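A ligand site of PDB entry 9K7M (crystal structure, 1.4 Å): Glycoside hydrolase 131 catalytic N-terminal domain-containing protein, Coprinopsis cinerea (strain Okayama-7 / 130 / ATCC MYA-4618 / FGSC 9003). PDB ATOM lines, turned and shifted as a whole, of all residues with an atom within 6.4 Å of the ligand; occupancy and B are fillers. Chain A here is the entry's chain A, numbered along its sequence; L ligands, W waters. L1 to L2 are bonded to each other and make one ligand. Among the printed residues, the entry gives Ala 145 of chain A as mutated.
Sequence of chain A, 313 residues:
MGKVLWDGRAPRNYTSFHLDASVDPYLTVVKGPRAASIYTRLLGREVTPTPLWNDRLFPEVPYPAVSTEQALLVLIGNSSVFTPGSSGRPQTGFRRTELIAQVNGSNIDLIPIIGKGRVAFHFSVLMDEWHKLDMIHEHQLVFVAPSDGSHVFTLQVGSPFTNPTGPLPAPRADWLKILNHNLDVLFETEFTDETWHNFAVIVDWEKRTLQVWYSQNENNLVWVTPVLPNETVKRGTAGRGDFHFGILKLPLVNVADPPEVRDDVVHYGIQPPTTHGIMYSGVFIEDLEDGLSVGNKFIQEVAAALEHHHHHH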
ATOM      1  N   PHE A  82      28.811 -29.831  -5.741  1.00  0.00           N
ATOM      2  CA  PHE A  82      28.481 -30.165  -7.114  1.00  0.00           C
ATOM      3  C   PHE A  82      29.463 -29.478  -8.068  1.00  0.00           C
ATOM      4  O   PHE A  82      29.692 -28.286  -7.974  1.00  0.00           O
ATOM      5  CB  PHE A  82      27.048 -29.736  -7.442  1.00  0.00           C
ATOM      6  CG  PHE A  82      26.645 -30.023  -8.866  1.00  0.00           C
ATOM      7  CD1 PHE A  82      26.596 -31.314  -9.358  1.00  0.00           C
ATOM      8  CD2 PHE A  82      26.318 -28.979  -9.717  1.00  0.00           C
ATOM      9  CE1 PHE A  82      26.172 -31.558 -10.663  1.00  0.00           C
ATOM     10  CE2 PHE A  82      25.911 -29.220 -11.022  1.00  0.00           C
ATOM     11  CZ  PHE A  82      25.878 -30.504 -11.489  1.00  0.00           C
ATOM     12  N   PRO A  84      29.555 -28.541 -12.012  1.00  0.00           N
ATOM     13  CA  PRO A  84      28.799 -28.501 -13.282  1.00  0.00           C
ATOM     14  C   PRO A  84      29.555 -29.137 -14.441  1.00  0.00           C
ATOM     15  O   PRO A  84      30.740 -28.912 -14.610  1.00  0.00           O
ATOM     16  CB  PRO A  84      28.583 -27.010 -13.581  1.00  0.00           C
ATOM     17  CG  PRO A  84      28.788 -26.351 -12.219  1.00  0.00           C
ATOM     18  CD  PRO A  84      29.848 -27.186 -11.550  1.00  0.00           C
ATOM     19  N   GLN A  91      30.804 -25.888  -6.938  1.00  0.00           N
ATOM     20  CA  GLN A  91      29.898 -24.996  -6.253  1.00  0.00           C
ATOM     21  C   GLN A  91      30.139 -25.051  -4.750  1.00  0.00           C
ATOM     22  O   GLN A  91      29.313 -25.562  -3.975  1.00  0.00           O
ATOM     23  CB  GLN A  91      28.465 -25.358  -6.615  1.00  0.00           C
ATOM     24  CG  GLN A  91      28.150 -25.279  -8.102  1.00  0.00           C
ATOM     25  CD  GLN A  91      26.672 -25.431  -8.372  1.00  0.00           C
ATOM     26  OE1 GLN A  91      25.982 -26.183  -7.677  1.00  0.00           O
ATOM     27  NE2 GLN A  91      26.180 -24.674  -9.334  1.00  0.00           N
ATOM     28  N   PHE A  94      27.625 -23.993  -1.923  1.00  0.00           N
ATOM     29  CA  PHE A  94      26.435 -24.787  -1.691  1.00  0.00           C
ATOM     30  C   PHE A  94      26.813 -26.133  -1.097  1.00  0.00           C
ATOM     31  O   PHE A  94      27.920 -26.616  -1.310  1.00  0.00           O
ATOM     32  CB  PHE A  94      25.709 -25.086  -3.000  1.00  0.00           C
ATOM     33  CG  PHE A  94      25.050 -23.939  -3.706  1.00  0.00           C
ATOM     34  CD1 PHE A  94      24.609 -22.802  -3.035  1.00  0.00           C
ATOM     35  CD2 PHE A  94      24.767 -24.031  -5.057  1.00  0.00           C
ATOM     36  CE1 PHE A  94      23.975 -21.772  -3.719  1.00  0.00           C
ATOM     37  CE2 PHE A  94      24.115 -23.011  -5.715  1.00  0.00           C
ATOM     38  CZ  PHE A  94      23.695 -21.896  -5.052  1.00  0.00           C
ATOM     39  N   ARG A  96      24.736 -29.723  -1.594  1.00  0.00           N
ATOM     40  CA  ARG A  96      23.510 -30.152  -2.247  1.00  0.00           C
ATOM     41  C   ARG A  96      23.571 -31.617  -2.655  1.00  0.00           C
ATOM     42  O   ARG A  96      24.611 -32.166  -3.017  1.00  0.00           O
ATOM     43  CB  ARG A  96      23.177 -29.234  -3.423  1.00  0.00           C
ATOM     44  CG  ARG A  96      24.099 -29.343  -4.615  1.00  0.00           C
ATOM     45  CD  ARG A  96      23.962 -28.145  -5.563  1.00  0.00           C
ATOM     46  NE  ARG A  96      22.643 -28.072  -6.234  1.00  0.00           N
ATOM     47  CZ  ARG A  96      22.443 -27.715  -7.495  1.00  0.00           C
ATOM     48  NH1 ARG A  96      21.254 -27.851  -8.049  1.00  0.00           N
ATOM     49  NH2 ARG A  96      23.429 -27.232  -8.241  1.00  0.00           N
ATOM     50  N   GLU A  98      20.483 -33.667  -4.897  1.00  0.00           N
ATOM     51  CA  GLU A  98      19.151 -33.623  -5.459  1.00  0.00           C
ATOM     52  C   GLU A  98      18.910 -34.824  -6.361  1.00  0.00           C
ATOM     53  O   GLU A  98      19.838 -35.407  -6.898  1.00  0.00           O
ATOM     54  CB  GLU A  98      18.986 -32.340  -6.259  1.00  0.00           C
ATOM     55  CG  GLU A  98      18.957 -31.118  -5.358  1.00  0.00           C
ATOM     56  CD  GLU A  98      19.495 -29.874  -6.014  1.00  0.00           C
ATOM     57  OE1 GLU A  98      19.224 -29.633  -7.202  1.00  0.00           O
ATOM     58  OE2 GLU A  98      20.316 -29.219  -5.354  1.00  0.00           O
ATOM     59  N   GLU A 138      19.552 -21.334   4.877  1.00  0.00           N
ATOM     60  CA  GLU A 138      18.455 -21.524   3.940  1.00  0.00           C
ATOM     61  C   GLU A 138      18.653 -22.851   3.212  1.00  0.00           C
ATOM     62  O   GLU A 138      19.732 -23.158   2.738  1.00  0.00           O
ATOM     63  CB  GLU A 138      18.432 -20.384   2.935  1.00  0.00           C
ATOM     64  CG  GLU A 138      17.388 -20.569   1.820  1.00  0.00           C
ATOM     65  CD  GLU A 138      17.268 -19.410   0.851  1.00  0.00           C
ATOM     66  OE1 GLU A 138      17.789 -18.301   1.126  1.00  0.00           O
ATOM     67  OE2 GLU A 138      16.662 -19.627  -0.230  1.00  0.00           O
ATOM     68  N   GLN A 140      16.765 -24.983   0.012  1.00  0.00           N
ATOM     69  CA  GLN A 140      15.809 -25.130  -1.075  1.00  0.00           C
ATOM     70  C   GLN A 140      15.644 -26.630  -1.287  1.00  0.00           C
ATOM     71  O   GLN A 140      16.594 -27.302  -1.667  1.00  0.00           O
ATOM     72  CB  GLN A 140      16.353 -24.398  -2.283  1.00  0.00           C
ATOM     73  CG  GLN A 140      16.472 -22.919  -2.041  1.00  0.00           C
ATOM     74  CD  GLN A 140      17.312 -22.153  -3.029  1.00  0.00           C
ATOM     75  OE1 GLN A 140      17.598 -22.612  -4.137  1.00  0.00           O
ATOM     76  NE2 GLN A 140      17.691 -20.964  -2.608  1.00  0.00           N
ATOM     77  N   PHE A 143      11.908 -27.800  -6.165  1.00  0.00           N
ATOM     78  CA  PHE A 143      11.691 -26.717  -7.100  1.00  0.00           C
ATOM     79  C   PHE A 143      11.614 -27.246  -8.531  1.00  0.00           C
ATOM     80  O   PHE A 143      12.120 -28.332  -8.819  1.00  0.00           O
ATOM     81  CB  PHE A 143      12.773 -25.631  -6.952  1.00  0.00           C
ATOM     82  CG  PHE A 143      14.197 -26.127  -6.907  1.00  0.00           C
ATOM     83  CD1 PHE A 143      14.912 -26.256  -8.083  1.00  0.00           C
ATOM     84  CD2 PHE A 143      14.832 -26.402  -5.693  1.00  0.00           C
ATOM     85  CE1 PHE A 143      16.244 -26.653  -8.072  1.00  0.00           C
ATOM     86  CE2 PHE A 143      16.159 -26.808  -5.686  1.00  0.00           C
ATOM     87  CZ  PHE A 143      16.852 -26.942  -6.878  1.00  0.00           C
ATOM     88  N   ALA A 145      13.089 -25.872 -12.006  1.00  0.00           N
ATOM     89  CA  ALA A 145      14.111 -24.918 -12.431  1.00  0.00           C
ATOM     90  C   ALA A 145      14.199 -24.839 -13.955  1.00  0.00           C
ATOM     91  O   ALA A 145      14.717 -25.761 -14.576  1.00  0.00           O
ATOM     92  CB  ALA A 145      15.444 -25.314 -11.853  1.00  0.00           C
ATOM     93  N   ASP A 148      17.576 -20.974 -16.750  1.00  0.00           N
ATOM     94  CA  ASP A 148      18.250 -19.828 -16.164  1.00  0.00           C
ATOM     95  C   ASP A 148      18.545 -20.040 -14.676  1.00  0.00           C
ATOM     96  O   ASP A 148      19.157 -19.170 -14.055  1.00  0.00           O
ATOM     97  CB  ASP A 148      17.502 -18.531 -16.417  1.00  0.00           C
ATOM     98  CG  ASP A 148      16.172 -18.400 -15.711  1.00  0.00           C
ATOM     99  OD1 ASP A 148      15.749 -19.390 -15.044  1.00  0.00           O
ATOM    100  OD2 ASP A 148      15.572 -17.319 -15.819  1.00  0.00           O
ATOM    101  N   GLY A 149      18.107 -21.159 -14.097  1.00  0.00           N
ATOM    102  CA  GLY A 149      18.393 -21.456 -12.697  1.00  0.00           C
ATOM    103  C   GLY A 149      17.402 -20.845 -11.710  1.00  0.00           C
ATOM    104  O   GLY A 149      17.551 -21.049 -10.496  1.00  0.00           O
ATOM    105  N   SER A 150      16.440 -20.068 -12.190  1.00  0.00           N
ATOM    106  CA  SER A 150      15.322 -19.597 -11.392  1.00  0.00           C
ATOM    107  C   SER A 150      14.463 -20.796 -10.975  1.00  0.00           C
ATOM    108  O   SER A 150      14.669 -21.893 -11.439  1.00  0.00           O
ATOM    109  CB  SER A 150      14.508 -18.545 -12.160  1.00  0.00           C
ATOM    110  OG  SER A 150      13.819 -19.124 -13.265  1.00  0.00           O
ATOM    111  N   HIS A 151      13.486 -20.562 -10.100  1.00  0.00           N
ATOM    112  CA  HIS A 151      12.593 -21.597  -9.613  1.00  0.00           C
ATOM    113  C   HIS A 151      11.148 -21.161  -9.797  1.00  0.00           C
ATOM    114  O   HIS A 151      10.705 -20.169  -9.226  1.00  0.00           O
ATOM    115  CB  HIS A 151      12.838 -21.865  -8.121  1.00  0.00           C
ATOM    116  CG  HIS A 151      14.195 -22.427  -7.838  1.00  0.00           C
ATOM    117  ND1 HIS A 151      14.645 -22.590  -6.542  1.00  0.00           N
ATOM    118  CD2 HIS A 151      15.154 -22.885  -8.623  1.00  0.00           C
ATOM    119  CE1 HIS A 151      15.861 -23.115  -6.597  1.00  0.00           C
ATOM    120  NE2 HIS A 151      16.221 -23.223  -7.841  1.00  0.00           N
ATOM    121  N   LEU A 183       9.975 -15.220  -5.310  1.00  0.00           N
ATOM    122  CA  LEU A 183      10.333 -15.482  -3.921  1.00  0.00           C
ATOM    123  C   LEU A 183       9.326 -14.941  -2.913  1.00  0.00           C
ATOM    124  O   LEU A 183       9.596 -14.982  -1.711  1.00  0.00           O
ATOM    125  CB  LEU A 183      11.747 -15.005  -3.588  1.00  0.00           C
ATOM    126  CG  LEU A 183      12.868 -15.459  -4.514  1.00  0.00           C
ATOM    127  CD1 LEU A 183      14.197 -14.969  -4.005  1.00  0.00           C
ATOM    128  CD2 LEU A 183      12.922 -16.967  -4.639  1.00  0.00           C
ATOM    129  N   HIS A 244      13.295 -30.863  -9.352  1.00  0.00           N
ATOM    130  CA  HIS A 244      14.330 -31.247  -8.383  1.00  0.00           C
ATOM    131  C   HIS A 244      13.719 -31.472  -7.005  1.00  0.00           C
ATOM    132  O   HIS A 244      12.860 -30.695  -6.590  1.00  0.00           O
ATOM    133  CB  HIS A 244      15.347 -30.120  -8.176  1.00  0.00           C
ATOM    134  CG  HIS A 244      16.186 -29.720  -9.353  1.00  0.00           C
ATOM    135  ND1 HIS A 244      17.553 -29.566  -9.225  1.00  0.00           N
ATOM    136  CD2 HIS A 244      15.875 -29.356 -10.626  1.00  0.00           C
ATOM    137  CE1 HIS A 244      18.011 -29.142 -10.402  1.00  0.00           C
ATOM    138  NE2 HIS A 244      17.033 -29.042 -11.265  1.00  0.00           N
ATOM    139  N   LEU A 248      19.243 -28.382  -1.160  1.00  0.00           N
ATOM    140  CA  LEU A 248      20.205 -27.393  -1.625  1.00  0.00           C
ATOM    141  C   LEU A 248      20.376 -26.372  -0.500  1.00  0.00           C
ATOM    142  O   LEU A 248      19.502 -25.548  -0.270  1.00  0.00           O
ATOM    143  CB  LEU A 248      19.761 -26.766  -2.960  1.00  0.00           C
ATOM    144  CG  LEU A 248      20.392 -25.449  -3.420  1.00  0.00           C
ATOM    145  CD1 LEU A 248      21.895 -25.396  -3.325  1.00  0.00           C
ATOM    146  CD2 LEU A 248      20.011 -25.170  -4.856  1.00  0.00           C
ATOM    147  N   LEU A 250      22.192 -23.252   1.196  1.00  0.00           N
ATOM    148  CA  LEU A 250      22.967 -22.041   0.954  1.00  0.00           C
ATOM    149  C   LEU A 250      23.886 -21.811   2.144  1.00  0.00           C
ATOM    150  O   LEU A 250      23.659 -22.296   3.256  1.00  0.00           O
ATOM    151  CB  LEU A 250      22.027 -20.856   0.753  1.00  0.00           C
ATOM    152  CG  LEU A 250      21.711 -20.578  -0.720  1.00  0.00           C
ATOM    153  CD1 LEU A 250      20.997 -21.755  -1.361  1.00  0.00           C
ATOM    154  CD2 LEU A 250      20.881 -19.314  -0.843  1.00  0.00           C
ATOM    155  N   ASP A 263      27.870 -12.041  -2.476  1.00  0.00           N
ATOM    156  CA  ASP A 263      26.565 -12.381  -3.009  1.00  0.00           C
ATOM    157  C   ASP A 263      26.628 -13.679  -3.809  1.00  0.00           C
ATOM    158  O   ASP A 263      25.585 -14.265  -4.089  1.00  0.00           O
ATOM    159  CB  ASP A 263      26.015 -11.259  -3.894  1.00  0.00           C
ATOM    160  CG  ASP A 263      25.678  -9.997  -3.129  1.00  0.00           C
ATOM    161  OD1 ASP A 263      24.934 -10.104  -2.129  1.00  0.00           O
ATOM    162  OD2 ASP A 263      26.197  -8.930  -3.509  1.00  0.00           O
ATOM    163  N   ASP A 264      27.819 -14.120  -4.216  1.00  0.00           N
ATOM    164  CA  ASP A 264      27.958 -15.308  -5.046  1.00  0.00           C
ATOM    165  C   ASP A 264      27.973 -16.537  -4.153  1.00  0.00           C
ATOM    166  O   ASP A 264      29.006 -17.175  -3.955  1.00  0.00           O
ATOM    167  CB  ASP A 264      29.214 -15.243  -5.925  1.00  0.00           C
ATOM    168  CG  ASP A 264      29.399 -16.469  -6.791  1.00  0.00           C
ATOM    169  OD1 ASP A 264      28.383 -17.199  -7.006  1.00  0.00           O
ATOM    170  OD2 ASP A 264      30.546 -16.727  -7.204  1.00  0.00           O
ATOM    171  N   VAL A 265      26.777 -16.914  -3.692  1.00  0.00           N
ATOM    172  CA  VAL A 265      26.560 -18.042  -2.817  1.00  0.00           C
ATOM    173  C   VAL A 265      26.895 -19.371  -3.486  1.00  0.00           C
ATOM    174  O   VAL A 265      27.001 -20.370  -2.791  1.00  0.00           O
ATOM    175  CB  VAL A 265      25.112 -18.034  -2.295  1.00  0.00           C
ATOM    176  CG1 VAL A 265      24.901 -16.863  -1.366  1.00  0.00           C
ATOM    177  CG2 VAL A 265      24.075 -18.030  -3.413  1.00  0.00           C
ATOM    178  N   VAL A 266      26.977 -19.413  -4.819  1.00  0.00           N
ATOM    179  CA  VAL A 266      27.347 -20.638  -5.498  1.00  0.00           C
ATOM    180  C   VAL A 266      28.763 -21.042  -5.109  1.00  0.00           C
ATOM    181  O   VAL A 266      29.061 -22.228  -4.999  1.00  0.00           O
ATOM    182  CB  VAL A 266      27.241 -20.494  -7.031  1.00  0.00           C
ATOM    183  CG1 VAL A 266      27.603 -21.796  -7.720  1.00  0.00           C
ATOM    184  CG2 VAL A 266      25.869 -20.056  -7.453  1.00  0.00           C
HETATM  185  C1  LIG L   1      22.196 -23.890 -11.061  1.00  0.00           C
HETATM  186  C2  LIG L   1      22.340 -22.375 -11.112  1.00  0.00           C
HETATM  187  C3  LIG L   1      22.358 -21.778  -9.712  1.00  0.00           C
HETATM  188  C4  LIG L   1      21.093 -22.253  -8.985  1.00  0.00           C
HETATM  189  C5  LIG L   1      20.987 -23.774  -8.980  1.00  0.00           C
HETATM  190  C6  LIG L   1      19.702 -24.259  -8.332  1.00  0.00           C
HETATM  191  O1  LIG L   1      23.351 -24.509 -10.484  1.00  0.00           O
HETATM  192  O2  LIG L   1      23.575 -22.103 -11.788  1.00  0.00           O
HETATM  193  O3  LIG L   1      22.400 -20.334  -9.772  1.00  0.00           O
HETATM  194  O4  LIG L   1      21.074 -21.886  -7.587  1.00  0.00           O
HETATM  195  O5  LIG L   1      21.022 -24.251 -10.326  1.00  0.00           O
HETATM  196  O6  LIG L   1      18.529 -23.964  -9.092  1.00  0.00           O
HETATM  197  C1  LG2 L   2      19.874 -20.534  -6.032  1.00  0.00           C
HETATM  198  C2  LG2 L   2      19.579 -19.102  -5.628  1.00  0.00           C
HETATM  199  C3  LG2 L   2      20.849 -18.266  -5.659  1.00  0.00           C
HETATM  200  C4  LG2 L   2      21.496 -18.403  -7.017  1.00  0.00           C
HETATM  201  C5  LG2 L   2      22.808 -17.631  -7.032  1.00  0.00           C
HETATM  202  C6  LG2 L   2      20.641 -20.562  -7.346  1.00  0.00           C
HETATM  203  O1  LG2 L   2      18.669 -21.267  -6.168  1.00  0.00           O
HETATM  204  O2  LG2 L   2      19.053 -19.096  -4.299  1.00  0.00           O
HETATM  205  O3  LG2 L   2      20.522 -16.907  -5.413  1.00  0.00           O
HETATM  206  O4  LG2 L   2      21.816 -19.760  -7.217  1.00  0.00           O
HETATM  207  O5  LG2 L   2      23.292 -17.709  -8.400  1.00  0.00           O
HETATM  208  O   HOH W   1      24.525 -19.286 -11.693  1.00  0.00           O
HETATM  209  O   HOH W   2      25.979 -23.585 -12.952  1.00  0.00           O
HETATM  210  O   HOH W   3      25.851 -16.471  -7.944  1.00  0.00           O
HETATM  211  O   HOH W   4      20.261 -18.792 -11.123  1.00  0.00           O
HETATM  212  O   HOH W   5      17.076 -20.085  -8.041  1.00  0.00           O
HETATM  213  O   HOH W   6      18.887 -15.670  -7.559  1.00  0.00           O
HETATM  214  O   HOH W   7      17.373 -17.129  -3.732  1.00  0.00           O
HETATM  215  O   HOH W   8      21.255 -15.974  -2.975  1.00  0.00           O
HETATM  216  O   HOH W   9      18.576 -25.813 -11.181  1.00  0.00           O
HETATM  217  O   HOH W  10      22.033 -16.607 -10.382  1.00  0.00           O
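Water W5 lies within hydrogen-bond range of O of Gly 149, O1 of LG2 L2 and NE2 of His 151. Water W3 bridges the side-chain carboxylate (OD1) of Asp 264 (2.8 Å) and an oxygen (O5) of LG2 L2 (2.9 Å). Water W4 lies within hydrogen-bond range of an oxygen (O3) of LIG L1 (3.0 Å) and the backbone carbonyl oxygen of Asp 148 (3.2 Å).
Merely in contact with the ligand: Arg 96 (3.5 Å), Phe 94 (3.6 Å), Leu 248 (3.6 Å), Val 266 (3.6 Å), Phe 143 (3.7 Å), Val 265 (3.9 Å) and Leu 250 (3.9 Å). Within 4 Å of the ligand: Gln 91, Phe 94, Arg 96, Gln 140, Phe 143, Gly 149, His 151, Leu 248, Leu 250, Val 265 and Val 266.
The side-chain amide oxygen (OE1) of Gln 140 sits at hydrogen-bond distance from an oxygen (O1) of LG2 L2 (2.7 Å). A ring nitrogen (NE2) of His 151 sits at hydrogen-bond distance from an oxygen (O6) of LIG L1, 2.7 Å away. An oxygen (O1) of LIG L1 is in hydrogen-bond range of the side-chain amide nitrogen (NE2) of Gln 91 (3.1 Å). The backbone carbonyl oxygen of Gly 149 lies within hydrogen-bond range of an oxygen (O6) of LIG L1 (3.4 Å).
N of Gln 140 sits at hydrogen-bond distance from O of Leu 248 (2.8 Å). NE2 of Gln 140 sits at hydrogen-bond distance from OE2 of Glu 138 (2.9 Å). The side-chain amide oxygen (OE1) of Gln 91 is in hydrogen-bond range of the guanidinium group (NH2) of Arg 96 (2.8 Å). The backbone NH of Gln 91 sits at hydrogen-bond distance from the backbone carbonyl oxygen of Phe 82. The guanidinium group (NE) of Arg 96 lies within salt-bridge range of the side-chain carboxylate (OE2) of Glu 98 (2.7 Å). The backbone NH (N) of Val 266 sits close to the side-chain carboxylate (OD1) of Asp 264, 3.4 Å away. The backbone carbonyl oxygen (O) of Phe 143 lies within hydrogen-bond range of the backbone NH (N) of His 244 (2.8 Å). The backbone carbonyl oxygen (O) of Glu 138 sits at hydrogen-bond distance from the backbone NH (N) of Leu 250, at 2.9 Å.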
